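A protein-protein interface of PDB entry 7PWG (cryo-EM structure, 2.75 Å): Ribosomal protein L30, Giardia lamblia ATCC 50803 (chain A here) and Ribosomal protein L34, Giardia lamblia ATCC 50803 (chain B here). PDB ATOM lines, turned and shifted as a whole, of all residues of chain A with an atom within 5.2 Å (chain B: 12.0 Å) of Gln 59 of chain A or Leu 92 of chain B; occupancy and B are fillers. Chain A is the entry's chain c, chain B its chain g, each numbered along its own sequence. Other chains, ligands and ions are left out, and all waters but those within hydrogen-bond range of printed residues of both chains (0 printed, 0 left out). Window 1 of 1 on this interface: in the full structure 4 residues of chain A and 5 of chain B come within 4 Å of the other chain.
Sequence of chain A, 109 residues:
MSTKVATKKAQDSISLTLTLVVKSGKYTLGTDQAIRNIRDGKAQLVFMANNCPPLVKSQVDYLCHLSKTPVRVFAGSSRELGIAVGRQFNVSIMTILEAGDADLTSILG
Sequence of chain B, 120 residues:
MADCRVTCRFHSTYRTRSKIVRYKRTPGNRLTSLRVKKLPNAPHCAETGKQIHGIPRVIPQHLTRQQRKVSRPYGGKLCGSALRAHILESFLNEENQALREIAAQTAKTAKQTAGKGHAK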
ATOM      1  N   ILE A  35     -18.637 -13.741 -17.999  1.00  0.00           N
ATOM      2  CA  ILE A  35     -17.505 -13.366 -18.841  1.00  0.00           C
ATOM      3  C   ILE A  35     -16.538 -14.532 -18.989  1.00  0.00           C
ATOM      4  O   ILE A  35     -16.096 -14.854 -20.095  1.00  0.00           O
ATOM      5  CB  ILE A  35     -16.800 -12.130 -18.271  1.00  0.00           C
ATOM      6  CG1 ILE A  35     -17.586 -10.863 -18.603  1.00  0.00           C
ATOM      7  CG2 ILE A  35     -15.374 -12.048 -18.791  1.00  0.00           C
ATOM      8  CD1 ILE A  35     -17.099  -9.670 -17.865  1.00  0.00           C
ATOM      9  N   LEU A  55     -22.237   0.362 -19.215  1.00  0.00           N
ATOM     10  CA  LEU A  55     -20.888  -0.023 -19.622  1.00  0.00           C
ATOM     11  C   LEU A  55     -20.732  -1.538 -19.635  1.00  0.00           C
ATOM     12  O   LEU A  55     -20.041  -2.086 -20.497  1.00  0.00           O
ATOM     13  CB  LEU A  55     -19.850   0.623 -18.701  1.00  0.00           C
ATOM     14  CG  LEU A  55     -18.377   0.781 -19.115  1.00  0.00           C
ATOM     15  CD1 LEU A  55     -17.636   1.622 -18.085  1.00  0.00           C
ATOM     16  CD2 LEU A  55     -17.655  -0.541 -19.268  1.00  0.00           C
ATOM     17  N   VAL A  56     -21.359  -2.230 -18.688  1.00  0.00           N
ATOM     18  CA  VAL A  56     -21.218  -3.678 -18.612  1.00  0.00           C
ATOM     19  C   VAL A  56     -21.961  -4.357 -19.755  1.00  0.00           C
ATOM     20  O   VAL A  56     -21.493  -5.357 -20.307  1.00  0.00           O
ATOM     21  CB  VAL A  56     -21.695  -4.180 -17.241  1.00  0.00           C
ATOM     22  CG1 VAL A  56     -21.250  -5.595 -17.026  1.00  0.00           C
ATOM     23  CG2 VAL A  56     -21.173  -3.269 -16.137  1.00  0.00           C
ATOM     24  N   LYS A  57     -23.136  -3.842 -20.112  1.00  0.00           N
ATOM     25  CA  LYS A  57     -23.892  -4.407 -21.222  1.00  0.00           C
ATOM     26  C   LYS A  57     -23.151  -4.259 -22.542  1.00  0.00           C
ATOM     27  O   LYS A  57     -23.167  -5.169 -23.376  1.00  0.00           O
ATOM     28  CB  LYS A  57     -25.259  -3.742 -21.312  1.00  0.00           C
ATOM     29  CG  LYS A  57     -26.018  -4.114 -22.564  1.00  0.00           C
ATOM     30  CD  LYS A  57     -27.225  -3.248 -22.742  1.00  0.00           C
ATOM     31  CE  LYS A  57     -27.944  -3.565 -24.030  1.00  0.00           C
ATOM     32  NZ  LYS A  57     -29.178  -2.765 -24.159  1.00  0.00           N
ATOM     33  N   SER A  58     -22.510  -3.111 -22.760  1.00  0.00           N
ATOM     34  CA  SER A  58     -21.735  -2.920 -23.978  1.00  0.00           C
ATOM     35  C   SER A  58     -20.641  -3.963 -24.099  1.00  0.00           C
ATOM     36  O   SER A  58     -20.403  -4.501 -25.184  1.00  0.00           O
ATOM     37  CB  SER A  58     -21.141  -1.517 -24.005  1.00  0.00           C
ATOM     38  OG  SER A  58     -22.152  -0.549 -24.195  1.00  0.00           O
ATOM     39  N   GLN A  59     -19.975  -4.271 -22.987  1.00  0.00           N
ATOM     40  CA  GLN A  59     -18.892  -5.246 -23.004  1.00  0.00           C
ATOM     41  C   GLN A  59     -19.405  -6.657 -23.255  1.00  0.00           C
ATOM     42  O   GLN A  59     -18.740  -7.453 -23.925  1.00  0.00           O
ATOM     43  CB  GLN A  59     -18.121  -5.182 -21.696  1.00  0.00           C
ATOM     44  CG  GLN A  59     -17.065  -6.236 -21.589  1.00  0.00           C
ATOM     45  CD  GLN A  59     -16.461  -6.305 -20.221  1.00  0.00           C
ATOM     46  OE1 GLN A  59     -16.883  -5.602 -19.311  1.00  0.00           O
ATOM     47  NE2 GLN A  59     -15.475  -7.169 -20.062  1.00  0.00           N
ATOM     48  N   VAL A  60     -20.577  -6.997 -22.719  1.00  0.00           N
ATOM     49  CA  VAL A  60     -21.098  -8.351 -22.895  1.00  0.00           C
ATOM     50  C   VAL A  60     -21.499  -8.588 -24.342  1.00  0.00           C
ATOM     51  O   VAL A  60     -21.281  -9.675 -24.886  1.00  0.00           O
ATOM     52  CB  VAL A  60     -22.267  -8.614 -21.929  1.00  0.00           C
ATOM     53  CG1 VAL A  60     -22.838  -9.983 -22.156  1.00  0.00           C
ATOM     54  CG2 VAL A  60     -21.791  -8.508 -20.510  1.00  0.00           C
ATOM     55  N   ASP A  61     -22.087  -7.582 -24.993  1.00  0.00           N
ATOM     56  CA  ASP A  61     -22.420  -7.719 -26.407  1.00  0.00           C
ATOM     57  C   ASP A  61     -21.170  -7.831 -27.272  1.00  0.00           C
ATOM     58  O   ASP A  61     -21.146  -8.609 -28.229  1.00  0.00           O
ATOM     59  CB  ASP A  61     -23.279  -6.546 -26.872  1.00  0.00           C
ATOM     60  CG  ASP A  61     -24.734  -6.679 -26.456  1.00  0.00           C
ATOM     61  OD1 ASP A  61     -25.277  -7.802 -26.517  1.00  0.00           O
ATOM     62  OD2 ASP A  61     -25.340  -5.655 -26.069  1.00  0.00           O
ATOM     63  N   TYR A  62     -20.127  -7.054 -26.969  1.00  0.00           N
ATOM     64  CA  TYR A  62     -18.907  -7.135 -27.765  1.00  0.00           C
ATOM     65  C   TYR A  62     -18.259  -8.505 -27.637  1.00  0.00           C
ATOM     66  O   TYR A  62     -17.864  -9.112 -28.638  1.00  0.00           O
ATOM     67  CB  TYR A  62     -17.919  -6.042 -27.367  1.00  0.00           C
ATOM     68  CG  TYR A  62     -16.919  -5.769 -28.460  1.00  0.00           C
ATOM     69  CD1 TYR A  62     -15.737  -6.485 -28.546  1.00  0.00           C
ATOM     70  CD2 TYR A  62     -17.185  -4.828 -29.443  1.00  0.00           C
ATOM     71  CE1 TYR A  62     -14.840  -6.245 -29.562  1.00  0.00           C
ATOM     72  CE2 TYR A  62     -16.297  -4.586 -30.460  1.00  0.00           C
ATOM     73  CZ  TYR A  62     -15.129  -5.290 -30.514  1.00  0.00           C
ATOM     74  OH  TYR A  62     -14.249  -5.031 -31.533  1.00  0.00           O
ATOM     75  N   LEU A  63     -18.158  -9.014 -26.410  1.00  0.00           N
ATOM     76  CA  LEU A  63     -17.618 -10.351 -26.209  1.00  0.00           C
ATOM     77  C   LEU A  63     -18.485 -11.418 -26.853  1.00  0.00           C
ATOM     78  O   LEU A  63     -17.989 -12.497 -27.183  1.00  0.00           O
ATOM     79  CB  LEU A  63     -17.479 -10.647 -24.720  1.00  0.00           C
ATOM     80  CG  LEU A  63     -16.354  -9.981 -23.947  1.00  0.00           C
ATOM     81  CD1 LEU A  63     -16.372 -10.499 -22.535  1.00  0.00           C
ATOM     82  CD2 LEU A  63     -15.030 -10.273 -24.609  1.00  0.00           C
ATOM     83  N   CYS A  64     -19.785 -11.158 -27.002  1.00  0.00           N
ATOM     84  CA  CYS A  64     -20.675 -12.164 -27.568  1.00  0.00           C
ATOM     85  C   CYS A  64     -20.492 -12.287 -29.072  1.00  0.00           C
ATOM     86  O   CYS A  64     -20.438 -13.399 -29.602  1.00  0.00           O
ATOM     87  CB  CYS A  64     -22.128 -11.840 -27.230  1.00  0.00           C
ATOM     88  SG  CYS A  64     -22.680 -12.500 -25.649  1.00  0.00           S
ATOM     89  N   SER B  81     -10.151   1.377 -10.169  1.00  0.00           N
ATOM     90  CA  SER B  81     -11.400   0.968 -10.797  1.00  0.00           C
ATOM     91  C   SER B  81     -11.905   2.013 -11.776  1.00  0.00           C
ATOM     92  O   SER B  81     -12.500   1.667 -12.801  1.00  0.00           O
ATOM     93  CB  SER B  81     -12.465   0.704  -9.738  1.00  0.00           C
ATOM     94  OG  SER B  81     -12.574  -0.676  -9.482  1.00  0.00           O
ATOM     95  N   LEU B  83     -10.019   3.944 -13.540  1.00  0.00           N
ATOM     96  CA  LEU B  83      -9.207   3.838 -14.744  1.00  0.00           C
ATOM     97  C   LEU B  83      -9.758   2.770 -15.673  1.00  0.00           C
ATOM     98  O   LEU B  83      -9.959   3.017 -16.865  1.00  0.00           O
ATOM     99  CB  LEU B  83      -7.758   3.535 -14.379  1.00  0.00           C
ATOM    100  CG  LEU B  83      -6.828   3.251 -15.558  1.00  0.00           C
ATOM    101  CD1 LEU B  83      -6.826   4.421 -16.528  1.00  0.00           C
ATOM    102  CD2 LEU B  83      -5.420   2.949 -15.080  1.00  0.00           C
ATOM    103  N   ARG B  84     -10.034   1.586 -15.134  1.00  0.00           N
ATOM    104  CA  ARG B  84     -10.519   0.481 -15.948  1.00  0.00           C
ATOM    105  C   ARG B  84     -11.840   0.811 -16.634  1.00  0.00           C
ATOM    106  O   ARG B  84     -12.113   0.312 -17.730  1.00  0.00           O
ATOM    107  CB  ARG B  84     -10.657  -0.758 -15.075  1.00  0.00           C
ATOM    108  CG  ARG B  84     -11.151  -1.981 -15.785  1.00  0.00           C
ATOM    109  CD  ARG B  84     -11.379  -3.091 -14.796  1.00  0.00           C
ATOM    110  NE  ARG B  84     -11.828  -4.310 -15.437  1.00  0.00           N
ATOM    111  CZ  ARG B  84     -13.101  -4.603 -15.652  1.00  0.00           C
ATOM    112  NH1 ARG B  84     -14.046  -3.767 -15.263  1.00  0.00           N
ATOM    113  NH2 ARG B  84     -13.430  -5.735 -16.256  1.00  0.00           N
ATOM    114  N   ALA B  85     -12.672   1.636 -16.011  1.00  0.00           N
ATOM    115  CA  ALA B  85     -13.933   2.014 -16.627  1.00  0.00           C
ATOM    116  C   ALA B  85     -13.743   3.055 -17.722  1.00  0.00           C
ATOM    117  O   ALA B  85     -14.493   3.052 -18.700  1.00  0.00           O
ATOM    118  CB  ALA B  85     -14.897   2.527 -15.561  1.00  0.00           C
ATOM    119  N   HIS B  86     -12.772   3.957 -17.568  1.00  0.00           N
ATOM    120  CA  HIS B  86     -12.440   4.886 -18.641  1.00  0.00           C
ATOM    121  C   HIS B  86     -11.851   4.158 -19.841  1.00  0.00           C
ATOM    122  O   HIS B  86     -12.121   4.526 -20.987  1.00  0.00           O
ATOM    123  CB  HIS B  86     -11.462   5.948 -18.151  1.00  0.00           C
ATOM    124  CG  HIS B  86     -12.106   7.105 -17.463  1.00  0.00           C
ATOM    125  ND1 HIS B  86     -12.735   8.119 -18.149  1.00  0.00           N
ATOM    126  CD2 HIS B  86     -12.190   7.428 -16.154  1.00  0.00           C
ATOM    127  CE1 HIS B  86     -13.196   9.007 -17.289  1.00  0.00           C
ATOM    128  NE2 HIS B  86     -12.877   8.612 -16.072  1.00  0.00           N
ATOM    129  N   ILE B  87     -11.026   3.142 -19.595  1.00  0.00           N
ATOM    130  CA  ILE B  87     -10.394   2.400 -20.679  1.00  0.00           C
ATOM    131  C   ILE B  87     -11.439   1.675 -21.510  1.00  0.00           C
ATOM    132  O   ILE B  87     -11.367   1.657 -22.743  1.00  0.00           O
ATOM    133  CB  ILE B  87      -9.345   1.427 -20.112  1.00  0.00           C
ATOM    134  CG1 ILE B  87      -8.245   2.193 -19.383  1.00  0.00           C
ATOM    135  CG2 ILE B  87      -8.771   0.557 -21.200  1.00  0.00           C
ATOM    136  CD1 ILE B  87      -7.314   1.306 -18.601  1.00  0.00           C
ATOM    137  N   LEU B  88     -12.423   1.063 -20.852  1.00  0.00           N
ATOM    138  CA  LEU B  88     -13.462   0.337 -21.574  1.00  0.00           C
ATOM    139  C   LEU B  88     -14.369   1.281 -22.347  1.00  0.00           C
ATOM    140  O   LEU B  88     -14.753   0.986 -23.482  1.00  0.00           O
ATOM    141  CB  LEU B  88     -14.286  -0.505 -20.606  1.00  0.00           C
ATOM    142  CG  LEU B  88     -13.874  -1.960 -20.440  1.00  0.00           C
ATOM    143  CD1 LEU B  88     -12.404  -2.044 -20.184  1.00  0.00           C
ATOM    144  CD2 LEU B  88     -14.628  -2.600 -19.302  1.00  0.00           C
ATOM    145  N   GLU B  89     -14.743   2.407 -21.748  1.00  0.00           N
ATOM    146  CA  GLU B  89     -15.587   3.354 -22.459  1.00  0.00           C
ATOM    147  C   GLU B  89     -14.893   3.867 -23.710  1.00  0.00           C
ATOM    148  O   GLU B  89     -15.485   3.900 -24.792  1.00  0.00           O
ATOM    149  CB  GLU B  89     -15.975   4.509 -21.547  1.00  0.00           C
ATOM    150  CG  GLU B  89     -17.149   4.208 -20.668  1.00  0.00           C
ATOM    151  CD  GLU B  89     -18.304   5.154 -20.895  1.00  0.00           C
ATOM    152  OE1 GLU B  89     -18.154   6.082 -21.720  1.00  0.00           O
ATOM    153  OE2 GLU B  89     -19.353   4.967 -20.247  1.00  0.00           O
ATOM    154  N   SER B  90     -13.620   4.241 -23.590  1.00  0.00           N
ATOM    155  CA  SER B  90     -12.880   4.709 -24.754  1.00  0.00           C
ATOM    156  C   SER B  90     -12.843   3.655 -25.856  1.00  0.00           C
ATOM    157  O   SER B  90     -13.199   3.931 -27.004  1.00  0.00           O
ATOM    158  CB  SER B  90     -11.468   5.106 -24.345  1.00  0.00           C
ATOM    159  OG  SER B  90     -10.685   5.390 -25.484  1.00  0.00           O
ATOM    160  N   PHE B  91     -12.430   2.437 -25.523  1.00  0.00           N
ATOM    161  CA  PHE B  91     -12.275   1.416 -26.551  1.00  0.00           C
ATOM    162  C   PHE B  91     -13.608   1.043 -27.195  1.00  0.00           C
ATOM    163  O   PHE B  91     -13.676   0.867 -28.415  1.00  0.00           O
ATOM    164  CB  PHE B  91     -11.586   0.179 -25.976  1.00  0.00           C
ATOM    165  CG  PHE B  91     -11.704  -1.025 -26.849  1.00  0.00           C
ATOM    166  CD1 PHE B  91     -11.203  -1.012 -28.139  1.00  0.00           C
ATOM    167  CD2 PHE B  91     -12.330  -2.173 -26.393  1.00  0.00           C
ATOM    168  CE1 PHE B  91     -11.332  -2.126 -28.956  1.00  0.00           C
ATOM    169  CE2 PHE B  91     -12.448  -3.287 -27.198  1.00  0.00           C
ATOM    170  CZ  PHE B  91     -11.952  -3.263 -28.482  1.00  0.00           C
ATOM    171  N   LEU B  92     -14.678   0.920 -26.405  1.00  0.00           N
ATOM    172  CA  LEU B  92     -15.951   0.436 -26.938  1.00  0.00           C
ATOM    173  C   LEU B  92     -16.703   1.484 -27.744  1.00  0.00           C
ATOM    174  O   LEU B  92     -17.437   1.128 -28.667  1.00  0.00           O
ATOM    175  CB  LEU B  92     -16.850  -0.061 -25.810  1.00  0.00           C
ATOM    176  CG  LEU B  92     -16.475  -1.378 -25.151  1.00  0.00           C
ATOM    177  CD1 LEU B  92     -17.392  -1.631 -23.984  1.00  0.00           C
ATOM    178  CD2 LEU B  92     -16.558  -2.508 -26.141  1.00  0.00           C
ATOM    179  N   ASN B  93     -16.582   2.760 -27.397  1.00  0.00           N
ATOM    180  CA  ASN B  93     -17.243   3.791 -28.188  1.00  0.00           C
ATOM    181  C   ASN B  93     -16.630   3.892 -29.574  1.00  0.00           C
ATOM    182  O   ASN B  93     -17.337   4.152 -30.554  1.00  0.00           O
ATOM    183  CB  ASN B  93     -17.165   5.138 -27.476  1.00  0.00           C
ATOM    184  CG  ASN B  93     -17.750   5.091 -26.087  1.00  0.00           C
ATOM    185  OD1 ASN B  93     -18.597   4.251 -25.786  1.00  0.00           O
ATOM    186  ND2 ASN B  93     -17.287   5.991 -25.219  1.00  0.00           N
ATOM    187  N   GLU B  94     -15.313   3.707 -29.672  1.00  0.00           N
ATOM    188  CA  GLU B  94     -14.664   3.666 -30.975  1.00  0.00           C
ATOM    189  C   GLU B  94     -15.201   2.525 -31.828  1.00  0.00           C
ATOM    190  O   GLU B  94     -15.257   2.640 -33.055  1.00  0.00           O
ATOM    191  CB  GLU B  94     -13.162   3.522 -30.796  1.00  0.00           C
ATOM    192  CG  GLU B  94     -12.366   3.869 -32.025  1.00  0.00           C
ATOM    193  CD  GLU B  94     -11.138   3.010 -32.160  1.00  0.00           C
ATOM    194  OE1 GLU B  94     -10.908   2.172 -31.262  1.00  0.00           O
ATOM    195  OE2 GLU B  94     -10.423   3.154 -33.172  1.00  0.00           O
ATOM    196  N   GLU B  95     -15.604   1.427 -31.191  1.00  0.00           N
ATOM    197  CA  GLU B  95     -16.168   0.257 -31.841  1.00  0.00           C
ATOM    198  C   GLU B  95     -17.632   0.424 -32.223  1.00  0.00           C
ATOM    199  O   GLU B  95     -18.175  -0.429 -32.932  1.00  0.00           O
ATOM    200  CB  GLU B  95     -16.028  -0.955 -30.917  1.00  0.00           C
ATOM    201  CG  GLU B  95     -14.615  -1.371 -30.683  1.00  0.00           C
ATOM    202  CD  GLU B  95     -13.941  -1.736 -31.973  1.00  0.00           C
ATOM    203  OE1 GLU B  95     -14.639  -2.269 -32.869  1.00  0.00           O
ATOM    204  OE2 GLU B  95     -12.729  -1.481 -32.110  1.00  0.00           O
ATOM    205  N   ASN B  96     -18.287   1.471 -31.753  1.00  0.00           N
ATOM    206  CA  ASN B  96     -19.686   1.698 -32.066  1.00  0.00           C
ATOM    207  C   ASN B  96     -19.939   2.989 -32.826  1.00  0.00           C
ATOM    208  O   ASN B  96     -20.907   3.059 -33.583  1.00  0.00           O
ATOM    209  CB  ASN B  96     -20.524   1.688 -30.777  1.00  0.00           C
ATOM    210  CG  ASN B  96     -20.419   0.378 -30.036  1.00  0.00           C
ATOM    211  OD1 ASN B  96     -19.958  -0.616 -30.589  1.00  0.00           O
ATOM    212  ND2 ASN B  96     -20.853   0.364 -28.787  1.00  0.00           N
ATOM    213  N   GLN B  97     -19.107   4.010 -32.652  1.00  0.00           N
ATOM    214  CA  GLN B  97     -19.224   5.178 -33.510  1.00  0.00           C
ATOM    215  C   GLN B  97     -18.716   4.887 -34.917  1.00  0.00           C
ATOM    216  O   GLN B  97     -19.061   5.610 -35.858  1.00  0.00           O
ATOM    217  CB  GLN B  97     -18.489   6.365 -32.879  1.00  0.00           C
ATOM    218  CG  GLN B  97     -18.293   7.567 -33.795  1.00  0.00           C
ATOM    219  CD  GLN B  97     -16.950   7.529 -34.507  1.00  0.00           C
ATOM    220  OE1 GLN B  97     -16.107   6.688 -34.203  1.00  0.00           O
ATOM    221  NE2 GLN B  97     -16.746   8.443 -35.449  1.00  0.00           N
ATOM    222  N   ALA B  98     -17.924   3.833 -35.081  1.00  0.00           N
ATOM    223  CA  ALA B  98     -17.466   3.388 -36.383  1.00  0.00           C
ATOM    224  C   ALA B  98     -17.691   1.889 -36.498  1.00  0.00           C
ATOM    225  O   ALA B  98     -17.743   1.177 -35.493  1.00  0.00           O
ATOM    226  CB  ALA B  98     -15.993   3.725 -36.615  1.00  0.00           C
ATOM    227  N   LEU B  99     -17.843   1.422 -37.736  1.00  0.00           N
ATOM    228  CA  LEU B  99     -18.222   0.044 -38.044  1.00  0.00           C
ATOM    229  C   LEU B  99     -19.497  -0.355 -37.294  1.00  0.00           C
ATOM    230  O   LEU B  99     -19.527  -1.303 -36.509  1.00  0.00           O
ATOM    231  CB  LEU B  99     -17.071  -0.926 -37.758  1.00  0.00           C
ATOM    232  CG  LEU B  99     -16.501  -1.557 -39.035  1.00  0.00           C
ATOM    233  CD1 LEU B  99     -15.588  -0.587 -39.792  1.00  0.00           C
ATOM    234  CD2 LEU B  99     -15.804  -2.879 -38.771  1.00  0.00           C
ATOM    235  N   ARG B 100     -20.562   0.388 -37.590  1.00  0.00           N
ATOM    236  CA  ARG B 100     -21.837   0.343 -36.868  1.00  0.00           C
ATOM    237  C   ARG B 100     -21.637   0.739 -35.412  1.00  0.00           C
ATOM    238  O   ARG B 100     -22.493   1.391 -34.823  1.00  0.00           O
ATOM    239  CB  ARG B 100     -22.500  -1.039 -36.952  1.00  0.00           C
ATOM    240  CG  ARG B 100     -23.978  -1.067 -36.494  1.00  0.00           C
ATOM    241  CD  ARG B 100     -24.176  -1.237 -34.977  1.00  0.00           C
ATOM    242  NE  ARG B 100     -23.766  -2.553 -34.495  1.00  0.00           N
ATOM    243  CZ  ARG B 100     -24.021  -3.028 -33.279  1.00  0.00           C
ATOM    244  NH1 ARG B 100     -24.679  -2.298 -32.391  1.00  0.00           N
ATOM    245  NH2 ARG B 100     -23.606  -4.240 -32.942  1.00  0.00           N
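The side-chain hydroxyl of Tyr 62 of chain A is in hydrogen-bond range of the side-chain carboxylate of Glu 95 of chain B, at 3.1 Å.
The backbone carbonyl oxygen (O) of Glu 89 of chain B is in hydrogen-bond range of the side-chain amide nitrogen (ND2) of Asn 93 of chain B (2.8 Å).
CD1 of Leu 55 of chain A touches O of Ala 85 of chain B, at 3.5 Å. Leu 88 of chain B touches Leu 55 of chain A (CB to CD2, 3.6 Å). Leu 55 of chain A touches Glu 89 of chain B (CD1 to CG, 3.7 Å). CD1 of Leu 92 of chain B touches CB of Ser 58 of chain A (3.8 Å). Gln 59 of chain A touches Leu 88 of chain B. CD1 of Leu 92 of chain B touches N of Gln 59 of chain A, at 3.8 Å. Tyr 62 of chain A touches Leu 92 of chain B (CB to CD2, 3.98 Å).
Gln 59 of chain A touches two residues of chain B. Of the printed residues of chain A, Leu 92 of chain B touches Ser 58, Gln 59 and Tyr 62. No residue of chain B comes within 4 Å of Ile 35 of chain A. Leu 55 of chain A touches just these residues of chain B: Ala 85 (3.5 Å), Leu 88 (3.6 Å) and Glu 89 (3.7 Å). No residue of chain B comes within 4 Å of Val 56 of chain A. No residue of chain B comes within 4 Å of Asp 61 of chain A. No residue of chain B comes within 4 Å of Leu 63 of chain A. Printed residues of chain A within 4 Å of Glu 89 of chain B: Leu 55. Of the printed residues of chain A, Ala 85 of chain B touches Leu 55 (3.5 Å). Printed residues of chain A within 4 Å of Leu 88 of chain B: Leu 55 and Gln 59. Asn 96 of chain B touches none of the printed residues of chain A. Arg 100 of chain B touches none of the printed residues of chain A. The nearest residue of chain B that does not touch Gln 59 of chain A is Arg 84 of chain B (4.6 Å). The nearest printed residue of chain A that does not touch Leu 92 of chain B is Leu 55 of chain A (4.4 Å).
Hydrophobic or aromatic side chains of chain A that line the printed part of chain B: Leu 55 and Tyr 62. Of the 19 printed residues of chain B, 5 touch a printed residue of chain A. Among the printed residues, 8 pairs touch across the chains.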
